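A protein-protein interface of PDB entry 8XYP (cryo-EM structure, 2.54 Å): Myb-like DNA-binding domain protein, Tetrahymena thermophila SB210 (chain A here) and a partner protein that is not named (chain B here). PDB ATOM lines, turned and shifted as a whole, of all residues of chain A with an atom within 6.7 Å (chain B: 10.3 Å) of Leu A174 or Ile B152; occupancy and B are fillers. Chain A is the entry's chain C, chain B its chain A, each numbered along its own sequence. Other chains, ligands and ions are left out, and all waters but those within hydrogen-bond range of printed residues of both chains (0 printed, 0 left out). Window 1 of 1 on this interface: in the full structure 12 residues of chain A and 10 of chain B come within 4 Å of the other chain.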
ATOM      1  N   LEU A 157     -11.831  16.408  -8.300  1.00  0.00           N
ATOM      2  CA  LEU A 157     -11.421  15.797  -9.559  1.00  0.00           C
ATOM      3  C   LEU A 157     -11.656  16.728 -10.742  1.00  0.00           C
ATOM      4  O   LEU A 157     -11.100  16.503 -11.824  1.00  0.00           O
ATOM      5  CB  LEU A 157     -12.152  14.472  -9.764  1.00  0.00           C
ATOM      6  CG  LEU A 157     -11.377  13.223  -9.337  1.00  0.00           C
ATOM      7  CD1 LEU A 157     -11.450  13.034  -7.831  1.00  0.00           C
ATOM      8  CD2 LEU A 157     -11.895  11.992 -10.055  1.00  0.00           C
ATOM      9  N   ILE A 160      -8.506  18.733 -11.738  1.00  0.00           N
ATOM     10  CA  ILE A 160      -7.416  17.875 -12.182  1.00  0.00           C
ATOM     11  C   ILE A 160      -7.784  17.042 -13.400  1.00  0.00           C
ATOM     12  O   ILE A 160      -6.910  16.373 -13.968  1.00  0.00           O
ATOM     13  CB  ILE A 160      -6.942  16.980 -11.020  1.00  0.00           C
ATOM     14  CG1 ILE A 160      -8.025  15.976 -10.645  1.00  0.00           C
ATOM     15  CG2 ILE A 160      -6.644  17.825  -9.800  1.00  0.00           C
ATOM     16  CD1 ILE A 160      -7.744  14.560 -11.021  1.00  0.00           C
ATOM     17  N   GLU A 161      -9.050  17.058 -13.822  1.00  0.00           N
ATOM     18  CA  GLU A 161      -9.481  16.339 -15.016  1.00  0.00           C
ATOM     19  C   GLU A 161      -9.784  17.284 -16.175  1.00  0.00           C
ATOM     20  O   GLU A 161     -10.547  16.929 -17.080  1.00  0.00           O
ATOM     21  CB  GLU A 161     -10.701  15.468 -14.704  1.00  0.00           C
ATOM     22  CG  GLU A 161     -10.769  14.175 -15.507  1.00  0.00           C
ATOM     23  CD  GLU A 161     -10.169  12.996 -14.778  1.00  0.00           C
ATOM     24  OE1 GLU A 161      -9.448  13.210 -13.783  1.00  0.00           O
ATOM     25  OE2 GLU A 161     -10.418  11.851 -15.209  1.00  0.00           O
ATOM     26  N   GLU A 169       0.838  16.408 -16.361  1.00  0.00           N
ATOM     27  CA  GLU A 169       0.385  17.262 -15.268  1.00  0.00           C
ATOM     28  C   GLU A 169      -0.885  16.723 -14.626  1.00  0.00           C
ATOM     29  O   GLU A 169      -1.083  16.889 -13.416  1.00  0.00           O
ATOM     30  CB  GLU A 169       0.191  18.700 -15.749  1.00  0.00           C
ATOM     31  CG  GLU A 169      -0.531  18.852 -17.063  1.00  0.00           C
ATOM     32  CD  GLU A 169      -0.091  20.097 -17.810  1.00  0.00           C
ATOM     33  OE1 GLU A 169       0.999  20.620 -17.498  1.00  0.00           O
ATOM     34  OE2 GLU A 169      -0.831  20.556 -18.703  1.00  0.00           O
ATOM     35  N   ILE A 170      -1.731  16.044 -15.406  1.00  0.00           N
ATOM     36  CA  ILE A 170      -2.882  15.348 -14.838  1.00  0.00           C
ATOM     37  C   ILE A 170      -2.416  14.290 -13.843  1.00  0.00           C
ATOM     38  O   ILE A 170      -2.942  14.187 -12.731  1.00  0.00           O
ATOM     39  CB  ILE A 170      -3.746  14.738 -15.957  1.00  0.00           C
ATOM     40  CG1 ILE A 170      -4.639  15.806 -16.587  1.00  0.00           C
ATOM     41  CG2 ILE A 170      -4.602  13.603 -15.432  1.00  0.00           C
ATOM     42  CD1 ILE A 170      -5.495  15.293 -17.723  1.00  0.00           C
ATOM     43  N   LEU A 171      -1.394  13.515 -14.215  1.00  0.00           N
ATOM     44  CA  LEU A 171      -0.890  12.474 -13.326  1.00  0.00           C
ATOM     45  C   LEU A 171      -0.182  13.049 -12.105  1.00  0.00           C
ATOM     46  O   LEU A 171      -0.262  12.463 -11.020  1.00  0.00           O
ATOM     47  CB  LEU A 171       0.035  11.535 -14.095  1.00  0.00           C
ATOM     48  CG  LEU A 171      -0.703  10.395 -14.795  1.00  0.00           C
ATOM     49  CD1 LEU A 171       0.063   9.921 -16.010  1.00  0.00           C
ATOM     50  CD2 LEU A 171      -0.936   9.251 -13.826  1.00  0.00           C
ATOM     51  N   THR A 172       0.514  14.181 -12.250  1.00  0.00           N
ATOM     52  CA  THR A 172       1.096  14.830 -11.076  1.00  0.00           C
ATOM     53  C   THR A 172       0.010  15.309 -10.124  1.00  0.00           C
ATOM     54  O   THR A 172       0.148  15.189  -8.901  1.00  0.00           O
ATOM     55  CB  THR A 172       1.989  16.009 -11.471  1.00  0.00           C
ATOM     56  OG1 THR A 172       1.218  16.986 -12.180  1.00  0.00           O
ATOM     57  CG2 THR A 172       3.166  15.558 -12.317  1.00  0.00           C
ATOM     58  N   HIS A 173      -1.079  15.862 -10.668  1.00  0.00           N
ATOM     59  CA  HIS A 173      -2.203  16.267  -9.832  1.00  0.00           C
ATOM     60  C   HIS A 173      -2.835  15.068  -9.132  1.00  0.00           C
ATOM     61  O   HIS A 173      -3.164  15.142  -7.941  1.00  0.00           O
ATOM     62  CB  HIS A 173      -3.234  17.007 -10.679  1.00  0.00           C
ATOM     63  CG  HIS A 173      -2.773  18.349 -11.156  1.00  0.00           C
ATOM     64  ND1 HIS A 173      -1.768  19.056 -10.534  1.00  0.00           N
ATOM     65  CD2 HIS A 173      -3.179  19.111 -12.200  1.00  0.00           C
ATOM     66  CE1 HIS A 173      -1.575  20.198 -11.172  1.00  0.00           C
ATOM     67  NE2 HIS A 173      -2.419  20.255 -12.186  1.00  0.00           N
ATOM     68  N   LEU A 174      -2.999  13.954  -9.857  1.00  0.00           N
ATOM     69  CA  LEU A 174      -3.505  12.723  -9.251  1.00  0.00           C
ATOM     70  C   LEU A 174      -2.610  12.254  -8.112  1.00  0.00           C
ATOM     71  O   LEU A 174      -3.098  11.862  -7.049  1.00  0.00           O
ATOM     72  CB  LEU A 174      -3.625  11.605 -10.288  1.00  0.00           C
ATOM     73  CG  LEU A 174      -4.899  11.224 -11.055  1.00  0.00           C
ATOM     74  CD1 LEU A 174      -6.050  10.930 -10.094  1.00  0.00           C
ATOM     75  CD2 LEU A 174      -5.311  12.200 -12.124  1.00  0.00           C
ATOM     76  N   TYR A 175      -1.292  12.282  -8.319  1.00  0.00           N
ATOM     77  CA  TYR A 175      -0.382  11.759  -7.306  1.00  0.00           C
ATOM     78  C   TYR A 175      -0.306  12.676  -6.092  1.00  0.00           C
ATOM     79  O   TYR A 175      -0.199  12.199  -4.955  1.00  0.00           O
ATOM     80  CB  TYR A 175       1.001  11.535  -7.912  1.00  0.00           C
ATOM     81  CG  TYR A 175       1.194  10.136  -8.447  1.00  0.00           C
ATOM     82  CD1 TYR A 175       1.271   9.052  -7.586  1.00  0.00           C
ATOM     83  CD2 TYR A 175       1.286   9.898  -9.812  1.00  0.00           C
ATOM     84  CE1 TYR A 175       1.442   7.772  -8.063  1.00  0.00           C
ATOM     85  CE2 TYR A 175       1.457   8.617 -10.301  1.00  0.00           C
ATOM     86  CZ  TYR A 175       1.534   7.558  -9.420  1.00  0.00           C
ATOM     87  OH  TYR A 175       1.705   6.279  -9.891  1.00  0.00           O
ATOM     88  N   ASN A 176      -0.367  13.994  -6.304  1.00  0.00           N
ATOM     89  CA  ASN A 176      -0.411  14.916  -5.174  1.00  0.00           C
ATOM     90  C   ASN A 176      -1.700  14.751  -4.374  1.00  0.00           C
ATOM     91  O   ASN A 176      -1.670  14.735  -3.135  1.00  0.00           O
ATOM     92  CB  ASN A 176      -0.255  16.355  -5.663  1.00  0.00           C
ATOM     93  CG  ASN A 176       1.197  16.734  -5.900  1.00  0.00           C
ATOM     94  OD1 ASN A 176       1.633  16.893  -7.040  1.00  0.00           O
ATOM     95  ND2 ASN A 176       1.953  16.878  -4.819  1.00  0.00           N
ATOM     96  N   LEU A 177      -2.838  14.610  -5.065  1.00  0.00           N
ATOM     97  CA  LEU A 177      -4.101  14.370  -4.373  1.00  0.00           C
ATOM     98  C   LEU A 177      -4.065  13.042  -3.625  1.00  0.00           C
ATOM     99  O   LEU A 177      -4.582  12.941  -2.506  1.00  0.00           O
ATOM    100  CB  LEU A 177      -5.257  14.408  -5.377  1.00  0.00           C
ATOM    101  CG  LEU A 177      -6.720  14.430  -4.911  1.00  0.00           C
ATOM    102  CD1 LEU A 177      -7.569  15.156  -5.941  1.00  0.00           C
ATOM    103  CD2 LEU A 177      -7.294  13.039  -4.666  1.00  0.00           C
ATOM    104  N   LYS A 178      -3.453  12.019  -4.229  1.00  0.00           N
ATOM    105  CA  LYS A 178      -3.305  10.725  -3.574  1.00  0.00           C
ATOM    106  C   LYS A 178      -2.463  10.836  -2.311  1.00  0.00           C
ATOM    107  O   LYS A 178      -2.801  10.244  -1.284  1.00  0.00           O
ATOM    108  CB  LYS A 178      -2.675   9.721  -4.540  1.00  0.00           C
ATOM    109  CG  LYS A 178      -2.515   8.322  -3.965  1.00  0.00           C
ATOM    110  CD  LYS A 178      -1.106   7.796  -4.165  1.00  0.00           C
ATOM    111  CE  LYS A 178      -0.843   6.580  -3.292  1.00  0.00           C
ATOM    112  NZ  LYS A 178      -0.140   6.939  -2.031  1.00  0.00           N
ATOM    113  N   ALA A 179      -1.363  11.592  -2.372  1.00  0.00           N
ATOM    114  CA  ALA A 179      -0.526  11.777  -1.191  1.00  0.00           C
ATOM    115  C   ALA A 179      -1.282  12.501  -0.083  1.00  0.00           C
ATOM    116  O   ALA A 179      -1.208  12.107   1.089  1.00  0.00           O
ATOM    117  CB  ALA A 179       0.745  12.540  -1.560  1.00  0.00           C
ATOM    118  N   ILE A 181      -4.610  12.658   0.401  1.00  0.00           N
ATOM    119  CA  ILE A 181      -5.664  11.831   0.980  1.00  0.00           C
ATOM    120  C   ILE A 181      -5.110  10.609   1.708  1.00  0.00           C
ATOM    121  O   ILE A 181      -5.758  10.115   2.636  1.00  0.00           O
ATOM    122  CB  ILE A 181      -6.699  11.421  -0.082  1.00  0.00           C
ATOM    123  CG1 ILE A 181      -6.103  10.449  -1.097  1.00  0.00           C
ATOM    124  CG2 ILE A 181      -7.289  12.652  -0.760  1.00  0.00           C
ATOM    125  CD1 ILE A 181      -7.116   9.920  -2.073  1.00  0.00           C
ATOM    126  N   VAL A 182      -3.917  10.127   1.352  1.00  0.00           N
ATOM    127  CA  VAL A 182      -3.272   9.088   2.150  1.00  0.00           C
ATOM    128  C   VAL A 182      -2.833   9.653   3.496  1.00  0.00           C
ATOM    129  O   VAL A 182      -2.946   8.985   4.534  1.00  0.00           O
ATOM    130  CB  VAL A 182      -2.102   8.464   1.361  1.00  0.00           C
ATOM    131  CG1 VAL A 182      -1.103   7.779   2.283  1.00  0.00           C
ATOM    132  CG2 VAL A 182      -2.635   7.460   0.351  1.00  0.00           C
ATOM    133  N   GLY B 144     -15.829   6.816   2.794  1.00  0.00           N
ATOM    134  CA  GLY B 144     -15.900   7.696   1.638  1.00  0.00           C
ATOM    135  C   GLY B 144     -14.533   8.095   1.116  1.00  0.00           C
ATOM    136  O   GLY B 144     -14.312   8.152  -0.097  1.00  0.00           O
ATOM    137  N   LEU B 145     -13.593   8.369   2.023  1.00  0.00           N
ATOM    138  CA  LEU B 145     -12.238   8.705   1.598  1.00  0.00           C
ATOM    139  C   LEU B 145     -11.538   7.492   0.995  1.00  0.00           C
ATOM    140  O   LEU B 145     -10.741   7.625   0.064  1.00  0.00           O
ATOM    141  CB  LEU B 145     -11.442   9.271   2.773  1.00  0.00           C
ATOM    142  CG  LEU B 145     -11.080  10.756   2.676  1.00  0.00           C
ATOM    143  CD1 LEU B 145     -10.084  11.146   3.757  1.00  0.00           C
ATOM    144  CD2 LEU B 145     -10.532  11.090   1.295  1.00  0.00           C
ATOM    145  N   GLN B 146     -11.834   6.295   1.512  1.00  0.00           N
ATOM    146  CA  GLN B 146     -11.305   5.075   0.907  1.00  0.00           C
ATOM    147  C   GLN B 146     -11.848   4.876  -0.505  1.00  0.00           C
ATOM    148  O   GLN B 146     -11.106   4.491  -1.419  1.00  0.00           O
ATOM    149  CB  GLN B 146     -11.638   3.871   1.793  1.00  0.00           C
ATOM    150  CG  GLN B 146     -11.629   2.516   1.087  1.00  0.00           C
ATOM    151  CD  GLN B 146     -10.232   1.977   0.831  1.00  0.00           C
ATOM    152  OE1 GLN B 146      -9.457   2.551   0.064  1.00  0.00           O
ATOM    153  NE2 GLN B 146      -9.903   0.864   1.477  1.00  0.00           N
ATOM    154  N   GLY B 147     -13.141   5.144  -0.702  1.00  0.00           N
ATOM    155  CA  GLY B 147     -13.708   5.063  -2.039  1.00  0.00           C
ATOM    156  C   GLY B 147     -13.121   6.093  -2.986  1.00  0.00           C
ATOM    157  O   GLY B 147     -12.881   5.804  -4.163  1.00  0.00           O
ATOM    158  N   LEU B 148     -12.875   7.306  -2.485  1.00  0.00           N
ATOM    159  CA  LEU B 148     -12.226   8.327  -3.302  1.00  0.00           C
ATOM    160  C   LEU B 148     -10.794   7.926  -3.643  1.00  0.00           C
ATOM    161  O   LEU B 148     -10.317   8.198  -4.751  1.00  0.00           O
ATOM    162  CB  LEU B 148     -12.268   9.676  -2.579  1.00  0.00           C
ATOM    163  CG  LEU B 148     -11.876  10.969  -3.310  1.00  0.00           C
ATOM    164  CD1 LEU B 148     -10.402  11.310  -3.142  1.00  0.00           C
ATOM    165  CD2 LEU B 148     -12.252  10.911  -4.790  1.00  0.00           C
ATOM    166  N   LEU B 149     -10.099   7.280  -2.702  1.00  0.00           N
ATOM    167  CA  LEU B 149      -8.756   6.772  -2.963  1.00  0.00           C
ATOM    168  C   LEU B 149      -8.771   5.700  -4.044  1.00  0.00           C
ATOM    169  O   LEU B 149      -7.903   5.681  -4.923  1.00  0.00           O
ATOM    170  CB  LEU B 149      -8.145   6.229  -1.669  1.00  0.00           C
ATOM    171  CG  LEU B 149      -6.781   5.538  -1.730  1.00  0.00           C
ATOM    172  CD1 LEU B 149      -5.689   6.507  -2.141  1.00  0.00           C
ATOM    173  CD2 LEU B 149      -6.448   4.904  -0.388  1.00  0.00           C
ATOM    174  N   GLN B 150      -9.760   4.804  -3.999  1.00  0.00           N
ATOM    175  CA  GLN B 150      -9.906   3.809  -5.058  1.00  0.00           C
ATOM    176  C   GLN B 150     -10.191   4.473  -6.401  1.00  0.00           C
ATOM    177  O   GLN B 150      -9.649   4.061  -7.436  1.00  0.00           O
ATOM    178  CB  GLN B 150     -11.020   2.825  -4.703  1.00  0.00           C
ATOM    179  CG  GLN B 150     -10.604   1.730  -3.742  1.00  0.00           C
ATOM    180  CD  GLN B 150     -11.793   0.997  -3.154  1.00  0.00           C
ATOM    181  OE1 GLN B 150     -12.267   1.331  -2.069  1.00  0.00           O
ATOM    182  NE2 GLN B 150     -12.284  -0.007  -3.872  1.00  0.00           N
ATOM    183  N   ASP B 151     -11.037   5.508  -6.397  1.00  0.00           N
ATOM    184  CA  ASP B 151     -11.367   6.219  -7.628  1.00  0.00           C
ATOM    185  C   ASP B 151     -10.131   6.861  -8.246  1.00  0.00           C
ATOM    186  O   ASP B 151      -9.871   6.705  -9.447  1.00  0.00           O
ATOM    187  CB  ASP B 151     -12.438   7.274  -7.347  1.00  0.00           C
ATOM    188  CG  ASP B 151     -13.326   7.539  -8.548  1.00  0.00           C
ATOM    189  OD1 ASP B 151     -12.858   7.359  -9.692  1.00  0.00           O
ATOM    190  OD2 ASP B 151     -14.495   7.931  -8.345  1.00  0.00           O
ATOM    191  N   ILE B 152      -9.341   7.573  -7.438  1.00  0.00           N
ATOM    192  CA  ILE B 152      -8.147   8.205  -7.989  1.00  0.00           C
ATOM    193  C   ILE B 152      -7.073   7.182  -8.332  1.00  0.00           C
ATOM    194  O   ILE B 152      -6.247   7.449  -9.202  1.00  0.00           O
ATOM    195  CB  ILE B 152      -7.577   9.297  -7.062  1.00  0.00           C
ATOM    196  CG1 ILE B 152      -7.348   8.771  -5.648  1.00  0.00           C
ATOM    197  CG2 ILE B 152      -8.491  10.510  -7.054  1.00  0.00           C
ATOM    198  CD1 ILE B 152      -5.932   8.375  -5.348  1.00  0.00           C
ATOM    199  N   GLU B 153      -7.060   6.010  -7.688  1.00  0.00           N
ATOM    200  CA  GLU B 153      -6.151   4.954  -8.127  1.00  0.00           C
ATOM    201  C   GLU B 153      -6.527   4.443  -9.514  1.00  0.00           C
ATOM    202  O   GLU B 153      -5.650   4.205 -10.356  1.00  0.00           O
ATOM    203  CB  GLU B 153      -6.143   3.807  -7.118  1.00  0.00           C
ATOM    204  CG  GLU B 153      -5.243   4.035  -5.918  1.00  0.00           C
ATOM    205  CD  GLU B 153      -5.430   2.980  -4.846  1.00  0.00           C
ATOM    206  OE1 GLU B 153      -6.392   3.094  -4.058  1.00  0.00           O
ATOM    207  OE2 GLU B 153      -4.614   2.037  -4.790  1.00  0.00           O
ATOM    208  N   LYS B 154      -7.828   4.269  -9.771  1.00  0.00           N
ATOM    209  CA  LYS B 154      -8.264   3.885 -11.113  1.00  0.00           C
ATOM    210  C   LYS B 154      -7.930   4.964 -12.138  1.00  0.00           C
ATOM    211  O   LYS B 154      -7.513   4.654 -13.263  1.00  0.00           O
ATOM    212  CB  LYS B 154      -9.762   3.579 -11.126  1.00  0.00           C
ATOM    213  CG  LYS B 154     -10.197   2.497 -10.152  1.00  0.00           C
ATOM    214  CD  LYS B 154      -9.350   1.242 -10.289  1.00  0.00           C
ATOM    215  CE  LYS B 154      -9.656   0.248  -9.177  1.00  0.00           C
ATOM    216  NZ  LYS B 154      -9.001  -1.068  -9.407  1.00  0.00           N
ATOM    217  N   ARG B 155      -8.107   6.236 -11.770  1.00  0.00           N
ATOM    218  CA  ARG B 155      -7.740   7.319 -12.681  1.00  0.00           C
ATOM    219  C   ARG B 155      -6.231   7.368 -12.907  1.00  0.00           C
ATOM    220  O   ARG B 155      -5.777   7.670 -14.017  1.00  0.00           O
ATOM    221  CB  ARG B 155      -8.250   8.660 -12.155  1.00  0.00           C
ATOM    222  CG  ARG B 155      -9.745   8.698 -11.907  1.00  0.00           C
ATOM    223  CD  ARG B 155     -10.423   9.793 -12.710  1.00  0.00           C
ATOM    224  NE  ARG B 155     -10.252   9.630 -14.148  1.00  0.00           N
ATOM    225  CZ  ARG B 155     -10.908   8.749 -14.894  1.00  0.00           C
ATOM    226  NH1 ARG B 155     -11.800   7.925 -14.369  1.00  0.00           N
ATOM    227  NH2 ARG B 155     -10.669   8.700 -16.201  1.00  0.00           N
ATOM    228  N   ILE B 156      -5.445   7.064 -11.870  1.00  0.00           N
ATOM    229  CA  ILE B 156      -3.992   6.989 -12.005  1.00  0.00           C
ATOM    230  C   ILE B 156      -3.611   5.899 -12.995  1.00  0.00           C
ATOM    231  O   ILE B 156      -2.765   6.104 -13.866  1.00  0.00           O
ATOM    232  CB  ILE B 156      -3.332   6.763 -10.629  1.00  0.00           C
ATOM    233  CG1 ILE B 156      -3.068   8.094  -9.933  1.00  0.00           C
ATOM    234  CG2 ILE B 156      -2.023   5.989 -10.749  1.00  0.00           C
ATOM    235  CD1 ILE B 156      -2.866   7.973  -8.445  1.00  0.00           C
ATOM    236  N   LEU B 157      -4.245   4.729 -12.886  1.00  0.00           N
ATOM    237  CA  LEU B 157      -3.952   3.644 -13.818  1.00  0.00           C
ATOM    238  C   LEU B 157      -4.350   3.985 -15.252  1.00  0.00           C
ATOM    239  O   LEU B 157      -3.572   3.724 -16.180  1.00  0.00           O
ATOM    240  CB  LEU B 157      -4.656   2.360 -13.373  1.00  0.00           C
ATOM    241  CG  LEU B 157      -4.148   1.648 -12.115  1.00  0.00           C
ATOM    242  CD1 LEU B 157      -4.364   0.147 -12.232  1.00  0.00           C
ATOM    243  CD2 LEU B 157      -2.683   1.956 -11.830  1.00  0.00           C
ATOM    244  N   HIS B 158      -5.528   4.586 -15.443  1.00  0.00           N
ATOM    245  CA  HIS B 158      -5.971   4.958 -16.784  1.00  0.00           C
ATOM    246  C   HIS B 158      -5.048   6.003 -17.404  1.00  0.00           C
ATOM    247  O   HIS B 158      -4.641   5.878 -18.567  1.00  0.00           O
ATOM    248  CB  HIS B 158      -7.409   5.472 -16.733  1.00  0.00           C
ATOM    249  CG  HIS B 158      -7.794   6.315 -17.908  1.00  0.00           C
ATOM    250  ND1 HIS B 158      -8.307   7.587 -17.774  1.00  0.00           N
ATOM    251  CD2 HIS B 158      -7.755   6.065 -19.239  1.00  0.00           C
ATOM    252  CE1 HIS B 158      -8.557   8.088 -18.970  1.00  0.00           C
ATOM    253  NE2 HIS B 158      -8.231   7.185 -19.876  1.00  0.00           N
ATOM    254  N   TYR B 159      -4.690   7.037 -16.639  1.00  0.00           N
ATOM    255  CA  TYR B 159      -3.846   8.088 -17.193  1.00  0.00           C
ATOM    256  C   TYR B 159      -2.399   7.628 -17.319  1.00  0.00           C
ATOM    257  O   TYR B 159      -1.663   8.128 -18.173  1.00  0.00           O
ATOM    258  CB  TYR B 159      -3.957   9.351 -16.345  1.00  0.00           C
ATOM    259  CG  TYR B 159      -5.161  10.190 -16.704  1.00  0.00           C
ATOM    260  CD1 TYR B 159      -5.164  10.981 -17.843  1.00  0.00           C
ATOM    261  CD2 TYR B 159      -6.302  10.178 -15.912  1.00  0.00           C
ATOM    262  CE1 TYR B 159      -6.262  11.744 -18.179  1.00  0.00           C
ATOM    263  CE2 TYR B 159      -7.406  10.938 -16.241  1.00  0.00           C
ATOM    264  CZ  TYR B 159      -7.380  11.720 -17.375  1.00  0.00           C
ATOM    265  OH  TYR B 159      -8.475  12.481 -17.709  1.00  0.00           O
ATOM    266  N   LYS B 160      -1.978   6.664 -16.498  1.00  0.00           N
ATOM    267  CA  LYS B 160      -0.680   6.030 -16.683  1.00  0.00           C
ATOM    268  C   LYS B 160      -0.624   5.294 -18.008  1.00  0.00           C
ATOM    269  O   LYS B 160       0.368   5.384 -18.739  1.00  0.00           O
ATOM    270  CB  LYS B 160      -0.407   5.062 -15.532  1.00  0.00           C
ATOM    271  CG  LYS B 160       0.560   5.561 -14.478  1.00  0.00           C
ATOM    272  CD  LYS B 160       0.820   4.473 -13.448  1.00  0.00           C
ATOM    273  CE  LYS B 160       2.119   4.701 -12.706  1.00  0.00           C
ATOM    274  NZ  LYS B 160       2.582   3.483 -11.993  1.00  0.00           N
ATOM    275  N   LEU B 162      -2.517   5.996 -20.601  1.00  0.00           N
ATOM    276  CA  LEU B 162      -2.548   7.040 -21.624  1.00  0.00           C
ATOM    277  C   LEU B 162      -1.172   7.666 -21.829  1.00  0.00           C
ATOM    278  O   LEU B 162      -0.750   7.900 -22.969  1.00  0.00           O
ATOM    279  CB  LEU B 162      -3.571   8.112 -21.247  1.00  0.00           C
ATOM    280  CG  LEU B 162      -5.031   7.866 -21.630  1.00  0.00           C
ATOM    281  CD1 LEU B 162      -5.824   9.157 -21.528  1.00  0.00           C
ATOM    282  CD2 LEU B 162      -5.136   7.285 -23.030  1.00  0.00           C
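NE of Arg B155 lies within salt-bridge range of OE2 of Glu A161, at 2.5 Å. OH of Tyr B159 lies within hydrogen-bond range of OE2 of Glu A161 (3.2 Å).
ND1 of His B158 is in hydrogen-bond range of NH2 of Arg B155, 3.0 Å away.
Of the 18 printed residues of chain B, 7 touch a printed residue of chain A. Hydrophobic or aromatic side chains of chain B within 4 Å of the printed part of chain A: Leu B148, Leu B149, Ile B152, Ile B156 and Tyr B159. Among the printed residues, Asp or Glu carboxylates within 4 Å of a Lys or Arg side-chain nitrogen of the other chain: Glu A161 with Arg B155 (2.5 Å).
Leu B148 touches Leu A157. Tyr B159 touches Ile A170. CD2 of Leu A171 touches O of Ile B156, at 3.6 Å. CD1 of Leu A171 touches O of Tyr B159 (3.3 Å). CD2 of Leu A171 touches N of Lys B160, at 3.9 Å. CG2 of Ile B156 touches OH of Tyr A175, at 3.8 Å. CD1 of Leu B148 touches CD2 of Leu A177, 3.9 Å away. Leu A177 touches Ile B152. CD1 of Leu B148 touches CD1 of Ile A181, at 3.7 Å. Ile A181 touches Ile B152.
Ile A160 touches none of the printed residues of chain B. Of the printed residues of chain B, Ile A170 touches Tyr B159. Leu A174 touches three residues of chain B. Ile B152 touches five residues of chain A. Of the printed residues of chain A, Lys B160 touches Leu A171 (3.9 Å) and Tyr A175 (3.3 Å). The nearest printed residue of chain B that does not touch Leu A157 is Asp B151 (4.7 Å).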
